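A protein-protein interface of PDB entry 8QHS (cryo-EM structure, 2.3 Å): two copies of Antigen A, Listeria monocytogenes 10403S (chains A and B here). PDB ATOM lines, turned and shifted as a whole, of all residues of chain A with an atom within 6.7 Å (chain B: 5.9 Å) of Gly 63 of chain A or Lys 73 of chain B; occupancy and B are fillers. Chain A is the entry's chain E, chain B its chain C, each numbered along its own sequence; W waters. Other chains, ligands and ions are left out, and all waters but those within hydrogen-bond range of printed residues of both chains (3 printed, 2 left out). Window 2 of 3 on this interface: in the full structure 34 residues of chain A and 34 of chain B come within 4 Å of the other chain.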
ATOM      1  N   ASP A  60      22.083  -7.793 -18.068  1.00  0.00           N
ATOM      2  CA  ASP A  60      23.280  -7.877 -17.239  1.00  0.00           C
ATOM      3  C   ASP A  60      23.198  -9.042 -16.265  1.00  0.00           C
ATOM      4  O   ASP A  60      24.220  -9.487 -15.736  1.00  0.00           O
ATOM      5  CB  ASP A  60      23.488  -6.578 -16.465  1.00  0.00           C
ATOM      6  CG  ASP A  60      23.892  -5.430 -17.347  1.00  0.00           C
ATOM      7  OD1 ASP A  60      23.948  -5.608 -18.581  1.00  0.00           O
ATOM      8  OD2 ASP A  60      24.157  -4.341 -16.803  1.00  0.00           O
ATOM      9  N   THR A  61      21.992  -9.530 -16.000  1.00  0.00           N
ATOM     10  CA  THR A  61      21.812 -10.619 -15.052  1.00  0.00           C
ATOM     11  C   THR A  61      22.494 -11.883 -15.557  1.00  0.00           C
ATOM     12  O   THR A  61      22.239 -12.346 -16.670  1.00  0.00           O
ATOM     13  CB  THR A  61      20.323 -10.874 -14.818  1.00  0.00           C
ATOM     14  OG1 THR A  61      19.712  -9.687 -14.303  1.00  0.00           O
ATOM     15  CG2 THR A  61      20.128 -11.993 -13.825  1.00  0.00           C
ATOM     16  N   VAL A  62      23.369 -12.442 -14.724  1.00  0.00           N
ATOM     17  CA  VAL A  62      24.165 -13.603 -15.085  1.00  0.00           C
ATOM     18  C   VAL A  62      23.758 -14.773 -14.200  1.00  0.00           C
ATOM     19  O   VAL A  62      23.348 -14.603 -13.052  1.00  0.00           O
ATOM     20  CB  VAL A  62      25.680 -13.330 -14.957  1.00  0.00           C
ATOM     21  CG1 VAL A  62      26.332 -13.315 -16.325  1.00  0.00           C
ATOM     22  CG2 VAL A  62      25.928 -12.026 -14.237  1.00  0.00           C
ATOM     23  N   GLY A  63      23.866 -15.973 -14.756  1.00  0.00           N
ATOM     24  CA  GLY A  63      23.632 -17.178 -13.993  1.00  0.00           C
ATOM     25  C   GLY A  63      22.319 -17.874 -14.254  1.00  0.00           C
ATOM     26  O   GLY A  63      22.156 -19.022 -13.824  1.00  0.00           O
ATOM     27  N   GLY A  64      21.380 -17.230 -14.940  1.00  0.00           N
ATOM     28  CA  GLY A  64      20.132 -17.877 -15.278  1.00  0.00           C
ATOM     29  C   GLY A  64      19.041 -17.782 -14.240  1.00  0.00           C
ATOM     30  O   GLY A  64      18.039 -18.483 -14.355  1.00  0.00           O
ATOM     31  N   TRP A  65      19.199 -16.933 -13.234  1.00  0.00           N
ATOM     32  CA  TRP A  65      18.194 -16.741 -12.198  1.00  0.00           C
ATOM     33  C   TRP A  65      17.631 -15.337 -12.312  1.00  0.00           C
ATOM     34  O   TRP A  65      18.360 -14.400 -12.641  1.00  0.00           O
ATOM     35  CB  TRP A  65      18.783 -16.951 -10.805  1.00  0.00           C
ATOM     36  CG  TRP A  65      19.164 -18.352 -10.502  1.00  0.00           C
ATOM     37  CD1 TRP A  65      20.358 -18.941 -10.754  1.00  0.00           C
ATOM     38  CD2 TRP A  65      18.352 -19.342  -9.872  1.00  0.00           C
ATOM     39  NE1 TRP A  65      20.347 -20.237 -10.324  1.00  0.00           N
ATOM     40  CE2 TRP A  65      19.124 -20.510  -9.775  1.00  0.00           C
ATOM     41  CE3 TRP A  65      17.046 -19.357  -9.380  1.00  0.00           C
ATOM     42  CZ2 TRP A  65      18.636 -21.680  -9.216  1.00  0.00           C
ATOM     43  CZ3 TRP A  65      16.566 -20.513  -8.827  1.00  0.00           C
ATOM     44  CH2 TRP A  65      17.356 -21.662  -8.748  1.00  0.00           C
ATOM     45  N   LYS A  66      16.342 -15.195 -12.042  1.00  0.00           N
ATOM     46  CA  LYS A  66      15.738 -13.873 -11.999  1.00  0.00           C
ATOM     47  C   LYS A  66      16.294 -13.069 -10.832  1.00  0.00           C
ATOM     48  O   LYS A  66      16.694 -13.617  -9.804  1.00  0.00           O
ATOM     49  CB  LYS A  66      14.224 -13.991 -11.880  1.00  0.00           C
ATOM     50  CG  LYS A  66      13.567 -14.534 -13.110  1.00  0.00           C
ATOM     51  CD  LYS A  66      12.098 -14.770 -12.887  1.00  0.00           C
ATOM     52  CE  LYS A  66      11.448 -15.252 -14.157  1.00  0.00           C
ATOM     53  NZ  LYS A  66       9.993 -15.457 -13.998  1.00  0.00           N
ATOM     54  N   SER A  67      16.317 -11.755 -11.002  1.00  0.00           N
ATOM     55  CA  SER A  67      16.810 -10.835  -9.990  1.00  0.00           C
ATOM     56  C   SER A  67      15.637 -10.075  -9.389  1.00  0.00           C
ATOM     57  O   SER A  67      14.841  -9.479 -10.117  1.00  0.00           O
ATOM     58  CB  SER A  67      17.825  -9.870 -10.598  1.00  0.00           C
ATOM     59  OG  SER A  67      18.741  -9.421  -9.628  1.00  0.00           O
ATOM     60  N   LYS A  68      15.528 -10.101  -8.065  1.00  0.00           N
ATOM     61  CA  LYS A  68      14.401  -9.494  -7.373  1.00  0.00           C
ATOM     62  C   LYS A  68      14.877  -8.663  -6.195  1.00  0.00           C
ATOM     63  O   LYS A  68      15.893  -8.966  -5.570  1.00  0.00           O
ATOM     64  CB  LYS A  68      13.408 -10.556  -6.890  1.00  0.00           C
ATOM     65  CG  LYS A  68      12.693 -11.257  -8.013  1.00  0.00           C
ATOM     66  CD  LYS A  68      11.939 -12.470  -7.547  1.00  0.00           C
ATOM     67  CE  LYS A  68      11.386 -13.228  -8.731  1.00  0.00           C
ATOM     68  NZ  LYS A  68      10.690 -14.468  -8.337  1.00  0.00           N
ATOM     69  N   SER B  50      11.561 -23.124 -10.144  1.00  0.00           N
ATOM     70  CA  SER B  50      10.890 -23.217 -11.425  1.00  0.00           C
ATOM     71  C   SER B  50      11.702 -22.484 -12.479  1.00  0.00           C
ATOM     72  O   SER B  50      12.526 -21.624 -12.171  1.00  0.00           O
ATOM     73  CB  SER B  50       9.465 -22.655 -11.361  1.00  0.00           C
ATOM     74  OG  SER B  50       9.460 -21.291 -10.995  1.00  0.00           O
ATOM     75  N   LYS B  51      11.462 -22.849 -13.730  1.00  0.00           N
ATOM     76  CA  LYS B  51      12.107 -22.245 -14.883  1.00  0.00           C
ATOM     77  C   LYS B  51      11.031 -21.893 -15.896  1.00  0.00           C
ATOM     78  O   LYS B  51      10.076 -22.652 -16.074  1.00  0.00           O
ATOM     79  CB  LYS B  51      13.137 -23.198 -15.497  1.00  0.00           C
ATOM     80  CG  LYS B  51      13.884 -22.634 -16.680  1.00  0.00           C
ATOM     81  CD  LYS B  51      14.886 -23.626 -17.231  1.00  0.00           C
ATOM     82  CE  LYS B  51      15.772 -24.164 -16.134  1.00  0.00           C
ATOM     83  NZ  LYS B  51      16.930 -24.923 -16.654  1.00  0.00           N
ATOM     84  N   ASP B  52      11.179 -20.749 -16.552  1.00  0.00           N
ATOM     85  CA  ASP B  52      10.245 -20.383 -17.604  1.00  0.00           C
ATOM     86  C   ASP B  52      10.523 -21.170 -18.878  1.00  0.00           C
ATOM     87  O   ASP B  52      11.642 -21.616 -19.131  1.00  0.00           O
ATOM     88  CB  ASP B  52      10.319 -18.890 -17.907  1.00  0.00           C
ATOM     89  CG  ASP B  52       9.750 -18.045 -16.800  1.00  0.00           C
ATOM     90  OD1 ASP B  52       8.573 -18.248 -16.433  1.00  0.00           O
ATOM     91  OD2 ASP B  52      10.465 -17.149 -16.322  1.00  0.00           O
ATOM     92  N   GLY B  71      13.778 -20.787 -20.031  1.00  0.00           N
ATOM     93  CA  GLY B  71      13.981 -19.397 -19.692  1.00  0.00           C
ATOM     94  C   GLY B  71      14.753 -19.225 -18.399  1.00  0.00           C
ATOM     95  O   GLY B  71      15.621 -20.022 -18.043  1.00  0.00           O
ATOM     96  N   MET B  72      14.418 -18.161 -17.680  1.00  0.00           N
ATOM     97  CA  MET B  72      15.113 -17.857 -16.439  1.00  0.00           C
ATOM     98  C   MET B  72      14.495 -18.611 -15.267  1.00  0.00           C
ATOM     99  O   MET B  72      13.334 -19.016 -15.294  1.00  0.00           O
ATOM    100  CB  MET B  72      15.095 -16.357 -16.161  1.00  0.00           C
ATOM    101  CG  MET B  72      15.893 -15.540 -17.152  1.00  0.00           C
ATOM    102  SD  MET B  72      17.657 -15.889 -17.098  1.00  0.00           S
ATOM    103  CE  MET B  72      18.215 -14.615 -15.977  1.00  0.00           C
ATOM    104  N   LYS B  73      15.296 -18.786 -14.226  1.00  0.00           N
ATOM    105  CA  LYS B  73      14.902 -19.533 -13.044  1.00  0.00           C
ATOM    106  C   LYS B  73      14.503 -18.588 -11.920  1.00  0.00           C
ATOM    107  O   LYS B  73      14.973 -17.452 -11.850  1.00  0.00           O
ATOM    108  CB  LYS B  73      16.036 -20.444 -12.580  1.00  0.00           C
ATOM    109  CG  LYS B  73      16.304 -21.601 -13.508  1.00  0.00           C
ATOM    110  CD  LYS B  73      17.265 -22.590 -12.893  1.00  0.00           C
ATOM    111  CE  LYS B  73      18.646 -22.007 -12.739  1.00  0.00           C
ATOM    112  NZ  LYS B  73      19.260 -21.646 -14.028  1.00  0.00           N
ATOM    113  N   GLU B  74      13.625 -19.066 -11.051  1.00  0.00           N
ATOM    114  CA  GLU B  74      13.260 -18.372  -9.829  1.00  0.00           C
ATOM    115  C   GLU B  74      13.023 -19.406  -8.742  1.00  0.00           C
ATOM    116  O   GLU B  74      12.790 -20.580  -9.025  1.00  0.00           O
ATOM    117  CB  GLU B  74      12.018 -17.496 -10.018  1.00  0.00           C
ATOM    118  CG  GLU B  74      10.771 -18.254 -10.381  1.00  0.00           C
ATOM    119  CD  GLU B  74       9.588 -17.348 -10.637  1.00  0.00           C
ATOM    120  OE1 GLU B  74       9.795 -16.144 -10.884  1.00  0.00           O
ATOM    121  OE2 GLU B  74       8.444 -17.838 -10.588  1.00  0.00           O
ATOM    122  N   TRP B  75      13.102 -18.971  -7.494  1.00  0.00           N
ATOM    123  CA  TRP B  75      12.896 -19.877  -6.381  1.00  0.00           C
ATOM    124  C   TRP B  75      12.218 -19.155  -5.231  1.00  0.00           C
ATOM    125  O   TRP B  75      12.269 -17.931  -5.125  1.00  0.00           O
ATOM    126  CB  TRP B  75      14.212 -20.508  -5.902  1.00  0.00           C
ATOM    127  CG  TRP B  75      15.205 -19.554  -5.316  1.00  0.00           C
ATOM    128  CD1 TRP B  75      16.072 -18.762  -5.995  1.00  0.00           C
ATOM    129  CD2 TRP B  75      15.449 -19.316  -3.928  1.00  0.00           C
ATOM    130  NE1 TRP B  75      16.834 -18.039  -5.126  1.00  0.00           N
ATOM    131  CE2 TRP B  75      16.476 -18.364  -3.846  1.00  0.00           C
ATOM    132  CE3 TRP B  75      14.896 -19.814  -2.747  1.00  0.00           C
ATOM    133  CZ2 TRP B  75      16.962 -17.893  -2.631  1.00  0.00           C
ATOM    134  CZ3 TRP B  75      15.376 -19.347  -1.547  1.00  0.00           C
ATOM    135  CH2 TRP B  75      16.401 -18.397  -1.495  1.00  0.00           C
ATOM    136  N   GLY B 146      18.110 -14.068  -6.252  1.00  0.00           N
ATOM    137  CA  GLY B 146      19.051 -14.420  -7.282  1.00  0.00           C
ATOM    138  C   GLY B 146      19.177 -15.916  -7.359  1.00  0.00           C
ATOM    139  O   GLY B 146      18.184 -16.640  -7.305  1.00  0.00           O
HETATM  140  O   HOH W   1       8.530 -13.925 -11.304  1.00  0.00           O
HETATM  141  O   HOH W   2      21.301 -15.304 -17.252  1.00  0.00           O
HETATM  142  O   HOH W   3      17.750 -20.415 -16.559  1.00  0.00           O
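The side-chain amino group (NZ) of Lys 66 of chain A is in salt-bridge range of the side-chain carboxylate (OD2) of Asp 52 of chain B, 2.9 Å away.
NZ of Lys 66 of chain A is in salt-bridge range of OE1 of Glu 74 of chain B.
The side-chain amino group (NZ) of Lys 68 of chain A lies within salt-bridge range of the side-chain carboxylate (OE1) of Glu 74 of chain B.
The backbone carbonyl oxygen of Gly 64 of chain A lies within hydrogen-bond range of the backbone NH of Lys 73 of chain B (2.8 Å).
The backbone carbonyl oxygen (O) of Gly 64 of chain A lies close to the side-chain sulfur (SD) of Met 72 of chain B, at 3.8 Å.
The backbone carbonyl oxygen (O) of Lys 73 of chain B is in hydrogen-bond range of the backbone NH (N) of Lys 66 of chain A, 2.6 Å away.
Among the printed residues, pairs that only touch across the chains: Thr 61 of chain A with Met 72 of chain B (3.9 Å), Gly 63 of chain A with Lys 73 of chain B (3.9 Å), Trp 65 of chain A with Met 72 of chain B (3.3 Å), Trp 65 of chain A with Lys 73 of chain B (3.3 Å), Trp 65 of chain A with Glu 74 of chain B (3.7 Å), Trp 65 of chain A with Trp 75 of chain B (3.4 Å), Trp 65 of chain A with Gly 146 of chain B (3.6 Å), Lys 66 of chain A with Met 72 of chain B (3.9 Å) and Lys 66 of chain A with Gly 146 of chain B (3.5 Å).
No position is printed for both chains.
Of the 15 pairs that touch across the chains among the printed residues, none has its exchanged pair printed and touching as well.
The backbone NH (N) of Asp 52 of chain B sits at hydrogen-bond distance from the backbone carbonyl oxygen (O) of Met 72 of chain B (3.0 Å).
The backbone carbonyl oxygen (O) of Gly 146 of chain B sits at hydrogen-bond distance from the indole nitrogen (NE1) of Trp 75 of chain B (2.9 Å).
The backbone carbonyl oxygen of Ser 50 of chain B is in hydrogen-bond range of the backbone NH of Glu 74 of chain B, 3.0 Å away.
O of Asp 52 of chain B is in hydrogen-bond range of N of Gly 71 of chain B (2.5 Å).
Gly 63 of chain A touches one residue of chain B.
Of chain A, only Gly 63 (3.9 Å), Gly 64 (2.8 Å), Trp 65 (3.3 Å) and Lys 66 (2.6 Å) come within 4 Å of Lys 73 of chain B.
Of the printed residues of chain B, Gly 64 of chain A touches Met 72 (3.6 Å) and Lys 73 (2.8 Å).
Of the printed residues of chain A, Met 72 of chain B touches Thr 61, Gly 64, Trp 65 and Lys 66.
Of the printed residues of chain A, Asp 52 of chain B touches Lys 66 (2.9 Å).
Asp 60 of chain A touches none of the printed residues of chain B.
The nearest residue of chain B that does not touch Gly 63 of chain A is Met 72 of chain B (5.5 Å).
Of the 9 printed residues of chain A, 6 touch a printed residue of chain B.
Hydrophobic or aromatic side chains of chain A that line the printed part of chain B: Trp 65.
Hydrophobic or aromatic side chains of chain B that line the printed part of chain A: Met 72 and Trp 75.
Among the printed residues, Asp or Glu carboxylates within 4 Å of a Lys or Arg side-chain nitrogen of the other chain: Lys 66 of chain A with Asp 52 of chain B, Lys 66 of chain A with Glu 74 of chain B and Lys 68 of chain A with Glu 74 of chain B.
Water W1 bridges the side-chain carboxylate (OE1) of Glu 74 of chain B (2.6 Å) and the side-chain amino group (NZ) of Lys 66 of chain A (3.4 Å).
Water W3 lies within hydrogen-bond range of O of Gly 71 of chain B (2.6 Å), O of Gly 64 of chain A (2.9 Å) and NZ of Lys 73 of chain B (3.2 Å).
Water W2 lies within hydrogen-bond range of the backbone NH of Gly 64 of chain A (3.0 Å), the backbone carbonyl oxygen of Thr 61 of chain A (3.2 Å) and the side-chain sulfur of Met 72 of chain B (3.7 Å).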
